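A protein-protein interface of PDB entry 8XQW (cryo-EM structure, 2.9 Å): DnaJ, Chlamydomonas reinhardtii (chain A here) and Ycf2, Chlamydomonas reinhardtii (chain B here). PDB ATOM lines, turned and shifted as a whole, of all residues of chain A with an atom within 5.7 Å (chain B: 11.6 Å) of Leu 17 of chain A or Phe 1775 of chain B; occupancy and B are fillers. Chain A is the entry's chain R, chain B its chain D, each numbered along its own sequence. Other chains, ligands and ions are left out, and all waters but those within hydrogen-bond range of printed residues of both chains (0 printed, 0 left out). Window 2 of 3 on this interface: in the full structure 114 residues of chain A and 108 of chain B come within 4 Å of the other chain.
O of Pro 13 of chain A lies close to OD1 of Asp 16 of chain A (2.7 Å).
The backbone NH (N) of Ala 1780 of chain B is in hydrogen-bond range of the backbone carbonyl oxygen (O) of Phe 1775 of chain B, 3.4 Å away.
The side-chain hydroxyl of Tyr 14 of chain A sits at hydrogen-bond distance from the guanidinium group of Arg 24 of chain A (3.4 Å).
Trp 1776 of chain B touches Pro 13 of chain A (CH2 to O, 2.9 Å).
Tyr 14 of chain A touches Lys 1771 of chain B (OH to CD, 3.5 Å).
Leu 17 of chain A touches Phe 1775 of chain B.
Arg 24 of chain A touches Phe 1775 of chain B.
Leu 17 of chain A touches one residue of chain B.
Phe 1775 of chain B touches two residues of chain A.
No residue of chain B comes within 4 Å of Val 15 of chain A.
No residue of chain B comes within 4 Å of Leu 21 of chain A.
Arg 24 of chain A touches one residue of chain B.
Of the printed residues of chain B, Pro 13 of chain A touches Trp 1776.
Printed residues of chain A within 4 Å of Lys 1771 of chain B: Tyr 14.
Of the printed residues of chain A, Trp 1776 of chain B touches Pro 13 (2.9 Å).
Thr 1785 of chain B touches none of the printed residues of chain A.
The nearest residue of chain A that does not touch Phe 1775 of chain B is Tyr 14 of chain A (5.0 Å).
The nearest printed residue of chain B that does not touch Pro 13 of chain A is Gly 1772 of chain B (6.5 Å).
Hydrophobic or aromatic side chains of chain B within 4 Å of the printed part of chain A: Phe 1775 and Trp 1776.
Hydrophobic or aromatic side chains of chain A within 4 Å of the printed part of chain B: Pro 13, Tyr 14 and Leu 17.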
ATOM      1  N   PRO A  13     -15.603  14.460 -11.080  1.00  0.00           N
ATOM      2  CA  PRO A  13     -15.575  14.862 -12.492  1.00  0.00           C
ATOM      3  C   PRO A  13     -16.646  14.201 -13.338  1.00  0.00           C
ATOM      4  O   PRO A  13     -16.838  14.599 -14.491  1.00  0.00           O
ATOM      5  CB  PRO A  13     -14.170  14.444 -12.945  1.00  0.00           C
ATOM      6  CG  PRO A  13     -13.396  14.257 -11.699  1.00  0.00           C
ATOM      7  CD  PRO A  13     -14.364  13.786 -10.676  1.00  0.00           C
ATOM      8  N   TYR A  14     -17.346  13.199 -12.820  1.00  0.00           N
ATOM      9  CA  TYR A  14     -18.313  12.497 -13.646  1.00  0.00           C
ATOM     10  C   TYR A  14     -19.750  12.908 -13.377  1.00  0.00           C
ATOM     11  O   TYR A  14     -20.572  12.852 -14.295  1.00  0.00           O
ATOM     12  CB  TYR A  14     -18.181  10.988 -13.454  1.00  0.00           C
ATOM     13  CG  TYR A  14     -18.921  10.198 -14.496  1.00  0.00           C
ATOM     14  CD1 TYR A  14     -18.371   9.983 -15.746  1.00  0.00           C
ATOM     15  CD2 TYR A  14     -20.175   9.675 -14.232  1.00  0.00           C
ATOM     16  CE1 TYR A  14     -19.049   9.264 -16.702  1.00  0.00           C
ATOM     17  CE2 TYR A  14     -20.859   8.956 -15.182  1.00  0.00           C
ATOM     18  CZ  TYR A  14     -20.292   8.753 -16.414  1.00  0.00           C
ATOM     19  OH  TYR A  14     -20.975   8.036 -17.364  1.00  0.00           O
ATOM     20  N   VAL A  15     -20.076  13.315 -12.151  1.00  0.00           N
ATOM     21  CA  VAL A  15     -21.454  13.682 -11.845  1.00  0.00           C
ATOM     22  C   VAL A  15     -21.843  14.951 -12.589  1.00  0.00           C
ATOM     23  O   VAL A  15     -23.001  15.128 -12.985  1.00  0.00           O
ATOM     24  CB  VAL A  15     -21.643  13.830 -10.325  1.00  0.00           C
ATOM     25  CG1 VAL A  15     -20.620  14.778  -9.766  1.00  0.00           C
ATOM     26  CG2 VAL A  15     -23.046  14.312  -9.999  1.00  0.00           C
ATOM     27  N   ASP A  16     -20.883  15.850 -12.806  1.00  0.00           N
ATOM     28  CA  ASP A  16     -21.191  17.072 -13.537  1.00  0.00           C
ATOM     29  C   ASP A  16     -21.518  16.796 -14.996  1.00  0.00           C
ATOM     30  O   ASP A  16     -22.404  17.449 -15.556  1.00  0.00           O
ATOM     31  CB  ASP A  16     -20.033  18.064 -13.431  1.00  0.00           C
ATOM     32  CG  ASP A  16     -18.722  17.503 -13.951  1.00  0.00           C
ATOM     33  OD1 ASP A  16     -18.743  16.532 -14.733  1.00  0.00           O
ATOM     34  OD2 ASP A  16     -17.661  18.039 -13.569  1.00  0.00           O
ATOM     35  N   LEU A  17     -20.828  15.843 -15.620  1.00  0.00           N
ATOM     36  CA  LEU A  17     -21.152  15.486 -16.994  1.00  0.00           C
ATOM     37  C   LEU A  17     -22.532  14.854 -17.086  1.00  0.00           C
ATOM     38  O   LEU A  17     -23.183  14.939 -18.132  1.00  0.00           O
ATOM     39  CB  LEU A  17     -20.079  14.555 -17.551  1.00  0.00           C
ATOM     40  CG  LEU A  17     -20.311  13.886 -18.901  1.00  0.00           C
ATOM     41  CD1 LEU A  17     -19.008  13.812 -19.667  1.00  0.00           C
ATOM     42  CD2 LEU A  17     -20.883  12.493 -18.706  1.00  0.00           C
ATOM     43  N   MET A  18     -22.995  14.227 -16.009  1.00  0.00           N
ATOM     44  CA  MET A  18     -24.361  13.729 -15.961  1.00  0.00           C
ATOM     45  C   MET A  18     -25.352  14.820 -15.600  1.00  0.00           C
ATOM     46  O   MET A  18     -26.553  14.648 -15.824  1.00  0.00           O
ATOM     47  CB  MET A  18     -24.475  12.586 -14.953  1.00  0.00           C
ATOM     48  CG  MET A  18     -23.735  11.325 -15.345  1.00  0.00           C
ATOM     49  SD  MET A  18     -23.958  10.029 -14.119  1.00  0.00           S
ATOM     50  CE  MET A  18     -23.774  10.966 -12.611  1.00  0.00           C
ATOM     51  N   ARG A  19     -24.878  15.930 -15.035  1.00  0.00           N
ATOM     52  CA  ARG A  19     -25.751  17.080 -14.824  1.00  0.00           C
ATOM     53  C   ARG A  19     -26.198  17.681 -16.147  1.00  0.00           C
ATOM     54  O   ARG A  19     -27.293  18.245 -16.234  1.00  0.00           O
ATOM     55  CB  ARG A  19     -25.036  18.139 -13.988  1.00  0.00           C
ATOM     56  CG  ARG A  19     -25.356  18.110 -12.511  1.00  0.00           C
ATOM     57  CD  ARG A  19     -25.115  19.474 -11.894  1.00  0.00           C
ATOM     58  NE  ARG A  19     -25.130  19.442 -10.436  1.00  0.00           N
ATOM     59  CZ  ARG A  19     -24.039  19.451  -9.681  1.00  0.00           C
ATOM     60  NH1 ARG A  19     -22.841  19.487 -10.244  1.00  0.00           N
ATOM     61  NH2 ARG A  19     -24.145  19.424  -8.359  1.00  0.00           N
ATOM     62  N   SER A  20     -25.365  17.567 -17.179  1.00  0.00           N
ATOM     63  CA  SER A  20     -25.635  18.159 -18.479  1.00  0.00           C
ATOM     64  C   SER A  20     -26.171  17.162 -19.495  1.00  0.00           C
ATOM     65  O   SER A  20     -26.457  17.556 -20.629  1.00  0.00           O
ATOM     66  CB  SER A  20     -24.362  18.807 -19.031  1.00  0.00           C
ATOM     67  OG  SER A  20     -24.286  18.651 -20.434  1.00  0.00           O
ATOM     68  N   LEU A  21     -26.302  15.893 -19.130  1.00  0.00           N
ATOM     69  CA  LEU A  21     -26.791  14.859 -20.038  1.00  0.00           C
ATOM     70  C   LEU A  21     -27.681  13.907 -19.257  1.00  0.00           C
ATOM     71  O   LEU A  21     -27.163  12.978 -18.604  1.00  0.00           O
ATOM     72  CB  LEU A  21     -25.634  14.104 -20.683  1.00  0.00           C
ATOM     73  CG  LEU A  21     -24.545  14.908 -21.389  1.00  0.00           C
ATOM     74  CD1 LEU A  21     -23.337  14.043 -21.628  1.00  0.00           C
ATOM     75  CD2 LEU A  21     -25.060  15.450 -22.700  1.00  0.00           C
ATOM     76  N   ARG A  24     -27.205  10.152 -19.733  1.00  0.00           N
ATOM     77  CA  ARG A  24     -26.144   9.561 -18.930  1.00  0.00           C
ATOM     78  C   ARG A  24     -26.646   9.194 -17.543  1.00  0.00           C
ATOM     79  O   ARG A  24     -26.262   8.160 -16.992  1.00  0.00           O
ATOM     80  CB  ARG A  24     -24.962  10.518 -18.833  1.00  0.00           C
ATOM     81  CG  ARG A  24     -24.220  10.706 -20.132  1.00  0.00           C
ATOM     82  CD  ARG A  24     -24.246   9.443 -20.958  1.00  0.00           C
ATOM     83  NE  ARG A  24     -23.228   9.466 -21.998  1.00  0.00           N
ATOM     84  CZ  ARG A  24     -21.951   9.171 -21.791  1.00  0.00           C
ATOM     85  NH1 ARG A  24     -21.538   8.830 -20.580  1.00  0.00           N
ATOM     86  NH2 ARG A  24     -21.088   9.216 -22.795  1.00  0.00           N
ATOM     87  N   ILE B1766     -14.962   1.776 -10.592  1.00  0.00           N
ATOM     88  CA  ILE B1766     -14.098   1.311 -11.674  1.00  0.00           C
ATOM     89  C   ILE B1766     -14.617   1.808 -13.017  1.00  0.00           C
ATOM     90  O   ILE B1766     -13.848   2.283 -13.865  1.00  0.00           O
ATOM     91  CB  ILE B1766     -13.992  -0.220 -11.643  1.00  0.00           C
ATOM     92  CG1 ILE B1766     -13.504  -0.683 -10.278  1.00  0.00           C
ATOM     93  CG2 ILE B1766     -13.067  -0.705 -12.730  1.00  0.00           C
ATOM     94  CD1 ILE B1766     -13.602  -2.164 -10.084  1.00  0.00           C
ATOM     95  N   ALA B1767     -15.927   1.703 -13.235  1.00  0.00           N
ATOM     96  CA  ALA B1767     -16.496   2.205 -14.475  1.00  0.00           C
ATOM     97  C   ALA B1767     -16.313   3.709 -14.592  1.00  0.00           C
ATOM     98  O   ALA B1767     -16.033   4.225 -15.680  1.00  0.00           O
ATOM     99  CB  ALA B1767     -17.972   1.835 -14.561  1.00  0.00           C
ATOM    100  N   ARG B1768     -16.469   4.433 -13.481  1.00  0.00           N
ATOM    101  CA  ARG B1768     -16.241   5.873 -13.507  1.00  0.00           C
ATOM    102  C   ARG B1768     -14.806   6.191 -13.892  1.00  0.00           C
ATOM    103  O   ARG B1768     -14.561   7.115 -14.670  1.00  0.00           O
ATOM    104  CB  ARG B1768     -16.566   6.492 -12.153  1.00  0.00           C
ATOM    105  CG  ARG B1768     -18.034   6.710 -11.910  1.00  0.00           C
ATOM    106  CD  ARG B1768     -18.234   7.664 -10.761  1.00  0.00           C
ATOM    107  NE  ARG B1768     -19.297   7.217  -9.872  1.00  0.00           N
ATOM    108  CZ  ARG B1768     -19.508   7.714  -8.660  1.00  0.00           C
ATOM    109  NH1 ARG B1768     -18.728   8.675  -8.193  1.00  0.00           N
ATOM    110  NH2 ARG B1768     -20.500   7.250  -7.917  1.00  0.00           N
ATOM    111  N   GLN B1769     -13.846   5.436 -13.362  1.00  0.00           N
ATOM    112  CA  GLN B1769     -12.454   5.654 -13.739  1.00  0.00           C
ATOM    113  C   GLN B1769     -12.249   5.433 -15.230  1.00  0.00           C
ATOM    114  O   GLN B1769     -11.629   6.261 -15.905  1.00  0.00           O
ATOM    115  CB  GLN B1769     -11.536   4.735 -12.936  1.00  0.00           C
ATOM    116  CG  GLN B1769     -11.157   5.273 -11.567  1.00  0.00           C
ATOM    117  CD  GLN B1769     -10.582   4.203 -10.655  1.00  0.00           C
ATOM    118  OE1 GLN B1769      -9.872   3.303 -11.102  1.00  0.00           O
ATOM    119  NE2 GLN B1769     -10.897   4.295  -9.369  1.00  0.00           N
ATOM    120  N   GLU B1770     -12.763   4.325 -15.763  1.00  0.00           N
ATOM    121  CA  GLU B1770     -12.575   4.044 -17.185  1.00  0.00           C
ATOM    122  C   GLU B1770     -13.186   5.139 -18.054  1.00  0.00           C
ATOM    123  O   GLU B1770     -12.556   5.623 -19.005  1.00  0.00           O
ATOM    124  CB  GLU B1770     -13.175   2.684 -17.534  1.00  0.00           C
ATOM    125  CG  GLU B1770     -12.160   1.564 -17.739  1.00  0.00           C
ATOM    126  CD  GLU B1770     -11.425   1.152 -16.471  1.00  0.00           C
ATOM    127  OE1 GLU B1770     -11.687   1.722 -15.394  1.00  0.00           O
ATOM    128  OE2 GLU B1770     -10.574   0.242 -16.553  1.00  0.00           O
ATOM    129  N   LYS B1771     -14.414   5.552 -17.733  1.00  0.00           N
ATOM    130  CA  LYS B1771     -15.076   6.589 -18.516  1.00  0.00           C
ATOM    131  C   LYS B1771     -14.355   7.925 -18.394  1.00  0.00           C
ATOM    132  O   LYS B1771     -14.253   8.675 -19.370  1.00  0.00           O
ATOM    133  CB  LYS B1771     -16.529   6.728 -18.072  1.00  0.00           C
ATOM    134  CG  LYS B1771     -17.412   5.558 -18.454  1.00  0.00           C
ATOM    135  CD  LYS B1771     -18.580   5.423 -17.494  1.00  0.00           C
ATOM    136  CE  LYS B1771     -19.744   4.725 -18.154  1.00  0.00           C
ATOM    137  NZ  LYS B1771     -19.288   3.601 -19.008  1.00  0.00           N
ATOM    138  N   GLY B1772     -13.841   8.236 -17.203  1.00  0.00           N
ATOM    139  CA  GLY B1772     -13.094   9.468 -17.027  1.00  0.00           C
ATOM    140  C   GLY B1772     -11.809   9.495 -17.827  1.00  0.00           C
ATOM    141  O   GLY B1772     -11.453  10.522 -18.401  1.00  0.00           O
ATOM    142  N   THR B1773     -11.095   8.369 -17.885  1.00  0.00           N
ATOM    143  CA  THR B1773      -9.902   8.327 -18.730  1.00  0.00           C
ATOM    144  C   THR B1773     -10.262   8.426 -20.205  1.00  0.00           C
ATOM    145  O   THR B1773      -9.525   9.028 -20.990  1.00  0.00           O
ATOM    146  CB  THR B1773      -9.083   7.062 -18.476  1.00  0.00           C
ATOM    147  OG1 THR B1773      -9.703   5.942 -19.124  1.00  0.00           O
ATOM    148  CG2 THR B1773      -8.909   6.815 -16.994  1.00  0.00           C
ATOM    149  N   LEU B1774     -11.390   7.840 -20.606  1.00  0.00           N
ATOM    150  CA  LEU B1774     -11.769   7.947 -22.011  1.00  0.00           C
ATOM    151  C   LEU B1774     -12.148   9.376 -22.375  1.00  0.00           C
ATOM    152  O   LEU B1774     -11.863   9.840 -23.483  1.00  0.00           O
ATOM    153  CB  LEU B1774     -12.917   6.997 -22.327  1.00  0.00           C
ATOM    154  CG  LEU B1774     -13.346   7.062 -23.790  1.00  0.00           C
ATOM    155  CD1 LEU B1774     -13.206   5.701 -24.455  1.00  0.00           C
ATOM    156  CD2 LEU B1774     -14.762   7.590 -23.898  1.00  0.00           C
ATOM    157  N   PHE B1775     -12.781  10.093 -21.450  1.00  0.00           N
ATOM    158  CA  PHE B1775     -13.259  11.431 -21.770  1.00  0.00           C
ATOM    159  C   PHE B1775     -12.205  12.506 -21.539  1.00  0.00           C
ATOM    160  O   PHE B1775     -12.296  13.584 -22.132  1.00  0.00           O
ATOM    161  CB  PHE B1775     -14.504  11.756 -20.950  1.00  0.00           C
ATOM    162  CG  PHE B1775     -15.781  11.401 -21.636  1.00  0.00           C
ATOM    163  CD1 PHE B1775     -15.901  11.531 -23.009  1.00  0.00           C
ATOM    164  CD2 PHE B1775     -16.862  10.943 -20.911  1.00  0.00           C
ATOM    165  CE1 PHE B1775     -17.073  11.205 -23.642  1.00  0.00           C
ATOM    166  CE2 PHE B1775     -18.035  10.618 -21.538  1.00  0.00           C
ATOM    167  CZ  PHE B1775     -18.142  10.749 -22.905  1.00  0.00           C
ATOM    168  N   TRP B1776     -11.212  12.251 -20.688  1.00  0.00           N
ATOM    169  CA  TRP B1776     -10.287  13.294 -20.256  1.00  0.00           C
ATOM    170  C   TRP B1776      -8.833  12.978 -20.583  1.00  0.00           C
ATOM    171  O   TRP B1776      -8.013  13.892 -20.706  1.00  0.00           O
ATOM    172  CB  TRP B1776     -10.464  13.540 -18.754  1.00  0.00           C
ATOM    173  CG  TRP B1776     -11.304  14.739 -18.464  1.00  0.00           C
ATOM    174  CD1 TRP B1776     -11.077  16.011 -18.889  1.00  0.00           C
ATOM    175  CD2 TRP B1776     -12.534  14.774 -17.737  1.00  0.00           C
ATOM    176  NE1 TRP B1776     -12.069  16.845 -18.447  1.00  0.00           N
ATOM    177  CE2 TRP B1776     -12.980  16.110 -17.740  1.00  0.00           C
ATOM    178  CE3 TRP B1776     -13.296  13.810 -17.074  1.00  0.00           C
ATOM    179  CZ2 TRP B1776     -14.155  16.507 -17.108  1.00  0.00           C
ATOM    180  CZ3 TRP B1776     -14.462  14.205 -16.446  1.00  0.00           C
ATOM    181  CH2 TRP B1776     -14.881  15.542 -16.469  1.00  0.00           C
ATOM    182  N   ASP B1777      -8.481  11.701 -20.701  1.00  0.00           N
ATOM    183  CA  ASP B1777      -7.091  11.389 -21.001  1.00  0.00           C
ATOM    184  C   ASP B1777      -6.792  11.423 -22.492  1.00  0.00           C
ATOM    185  O   ASP B1777      -5.619  11.509 -22.868  1.00  0.00           O
ATOM    186  CB  ASP B1777      -6.709  10.031 -20.410  1.00  0.00           C
ATOM    187  CG  ASP B1777      -6.524  10.087 -18.897  1.00  0.00           C
ATOM    188  OD1 ASP B1777      -6.415  11.207 -18.354  1.00  0.00           O
ATOM    189  OD2 ASP B1777      -6.479   9.015 -18.256  1.00  0.00           O
ATOM    190  N   ILE B1778      -7.809  11.357 -23.347  1.00  0.00           N
ATOM    191  CA  ILE B1778      -7.587  11.462 -24.782  1.00  0.00           C
ATOM    192  C   ILE B1778      -8.402  12.612 -25.348  1.00  0.00           C
ATOM    193  O   ILE B1778      -7.881  13.455 -26.085  1.00  0.00           O
ATOM    194  CB  ILE B1778      -7.931  10.149 -25.506  1.00  0.00           C
ATOM    195  CG1 ILE B1778      -7.420   8.948 -24.715  1.00  0.00           C
ATOM    196  CG2 ILE B1778      -7.345  10.157 -26.903  1.00  0.00           C
ATOM    197  CD1 ILE B1778      -8.506   8.212 -23.972  1.00  0.00           C
ATOM    198  N   TRP B1779      -9.687  12.659 -25.008  1.00  0.00           N
ATOM    199  CA  TRP B1779     -10.561  13.626 -25.658  1.00  0.00           C
ATOM    200  C   TRP B1779     -10.273  15.044 -25.192  1.00  0.00           C
ATOM    201  O   TRP B1779     -10.415  15.993 -25.968  1.00  0.00           O
ATOM    202  CB  TRP B1779     -12.022  13.274 -25.410  1.00  0.00           C
ATOM    203  CG  TRP B1779     -12.591  12.267 -26.361  1.00  0.00           C
ATOM    204  CD1 TRP B1779     -13.456  11.266 -26.046  1.00  0.00           C
ATOM    205  CD2 TRP B1779     -12.347  12.157 -27.773  1.00  0.00           C
ATOM    206  NE1 TRP B1779     -13.772  10.542 -27.166  1.00  0.00           N
ATOM    207  CE2 TRP B1779     -13.102  11.065 -28.239  1.00  0.00           C
ATOM    208  CE3 TRP B1779     -11.569  12.874 -28.687  1.00  0.00           C
ATOM    209  CZ2 TRP B1779     -13.102  10.675 -29.570  1.00  0.00           C
ATOM    210  CZ3 TRP B1779     -11.570  12.480 -30.006  1.00  0.00           C
ATOM    211  CH2 TRP B1779     -12.331  11.392 -30.436  1.00  0.00           C
ATOM    212  N   ALA B1780      -9.856  15.211 -23.937  1.00  0.00           N
ATOM    213  CA  ALA B1780      -9.612  16.557 -23.430  1.00  0.00           C
ATOM    214  C   ALA B1780      -8.361  17.162 -24.047  1.00  0.00           C
ATOM    215  O   ALA B1780      -8.406  18.267 -24.595  1.00  0.00           O
ATOM    216  CB  ALA B1780      -9.502  16.536 -21.909  1.00  0.00           C
ATOM    217  N   ASP B1781      -7.234  16.454 -23.980  1.00  0.00           N
ATOM    218  CA  ASP B1781      -6.000  17.036 -24.495  1.00  0.00           C
ATOM    219  C   ASP B1781      -6.042  17.178 -26.012  1.00  0.00           C
ATOM    220  O   ASP B1781      -5.436  18.100 -26.570  1.00  0.00           O
ATOM    221  CB  ASP B1781      -4.788  16.212 -24.051  1.00  0.00           C
ATOM    222  CG  ASP B1781      -5.030  14.722 -24.128  1.00  0.00           C
ATOM    223  OD1 ASP B1781      -6.191  14.305 -23.948  1.00  0.00           O
ATOM    224  OD2 ASP B1781      -4.062  13.967 -24.365  1.00  0.00           O
ATOM    225  N   PHE B1782      -6.768  16.295 -26.699  1.00  0.00           N
ATOM    226  CA  PHE B1782      -6.876  16.424 -28.148  1.00  0.00           C
ATOM    227  C   PHE B1782      -7.582  17.716 -28.538  1.00  0.00           C
ATOM    228  O   PHE B1782      -7.092  18.475 -29.386  1.00  0.00           O
ATOM    229  CB  PHE B1782      -7.618  15.229 -28.730  1.00  0.00           C
ATOM    230  CG  PHE B1782      -8.000  15.408 -30.160  1.00  0.00           C
ATOM    231  CD1 PHE B1782      -7.033  15.402 -31.144  1.00  0.00           C
ATOM    232  CD2 PHE B1782      -9.320  15.600 -30.522  1.00  0.00           C
ATOM    233  CE1 PHE B1782      -7.371  15.571 -32.461  1.00  0.00           C
ATOM    234  CE2 PHE B1782      -9.665  15.768 -31.841  1.00  0.00           C
ATOM    235  CZ  PHE B1782      -8.688  15.754 -32.813  1.00  0.00           C
ATOM    236  N   LEU B1783      -8.742  17.984 -27.936  1.00  0.00           N
ATOM    237  CA  LEU B1783      -9.434  19.224 -28.252  1.00  0.00           C
ATOM    238  C   LEU B1783      -8.672  20.423 -27.706  1.00  0.00           C
ATOM    239  O   LEU B1783      -8.834  21.537 -28.205  1.00  0.00           O
ATOM    240  CB  LEU B1783     -10.871  19.194 -27.732  1.00  0.00           C
ATOM    241  CG  LEU B1783     -11.176  19.483 -26.272  1.00  0.00           C
ATOM    242  CD1 LEU B1783     -11.702  20.895 -26.184  1.00  0.00           C
ATOM    243  CD2 LEU B1783     -12.214  18.514 -25.750  1.00  0.00           C
ATOM    244  N   VAL B1784      -7.827  20.216 -26.692  1.00  0.00           N
ATOM    245  CA  VAL B1784      -6.910  21.277 -26.274  1.00  0.00           C
ATOM    246  C   VAL B1784      -5.952  21.630 -27.406  1.00  0.00           C
ATOM    247  O   VAL B1784      -5.721  22.809 -27.706  1.00  0.00           O
ATOM    248  CB  VAL B1784      -6.142  20.853 -25.009  1.00  0.00           C
ATOM    249  CG1 VAL B1784      -4.807  21.564 -24.941  1.00  0.00           C
ATOM    250  CG2 VAL B1784      -6.956  21.146 -23.772  1.00  0.00           C
ATOM    251  N   THR B1785      -5.365  20.610 -28.033  1.00  0.00           N
ATOM    252  CA  THR B1785      -4.485  20.843 -29.175  1.00  0.00           C
ATOM    253  C   THR B1785      -5.238  21.547 -30.299  1.00  0.00           C
ATOM    254  O   THR B1785      -4.726  22.488 -30.921  1.00  0.00           O
ATOM    255  CB  THR B1785      -3.894  19.521 -29.660  1.00  0.00           C
ATOM    256  OG1 THR B1785      -3.062  18.968 -28.634  1.00  0.00           O
ATOM    257  CG2 THR B1785      -3.068  19.731 -30.912  1.00  0.00           C
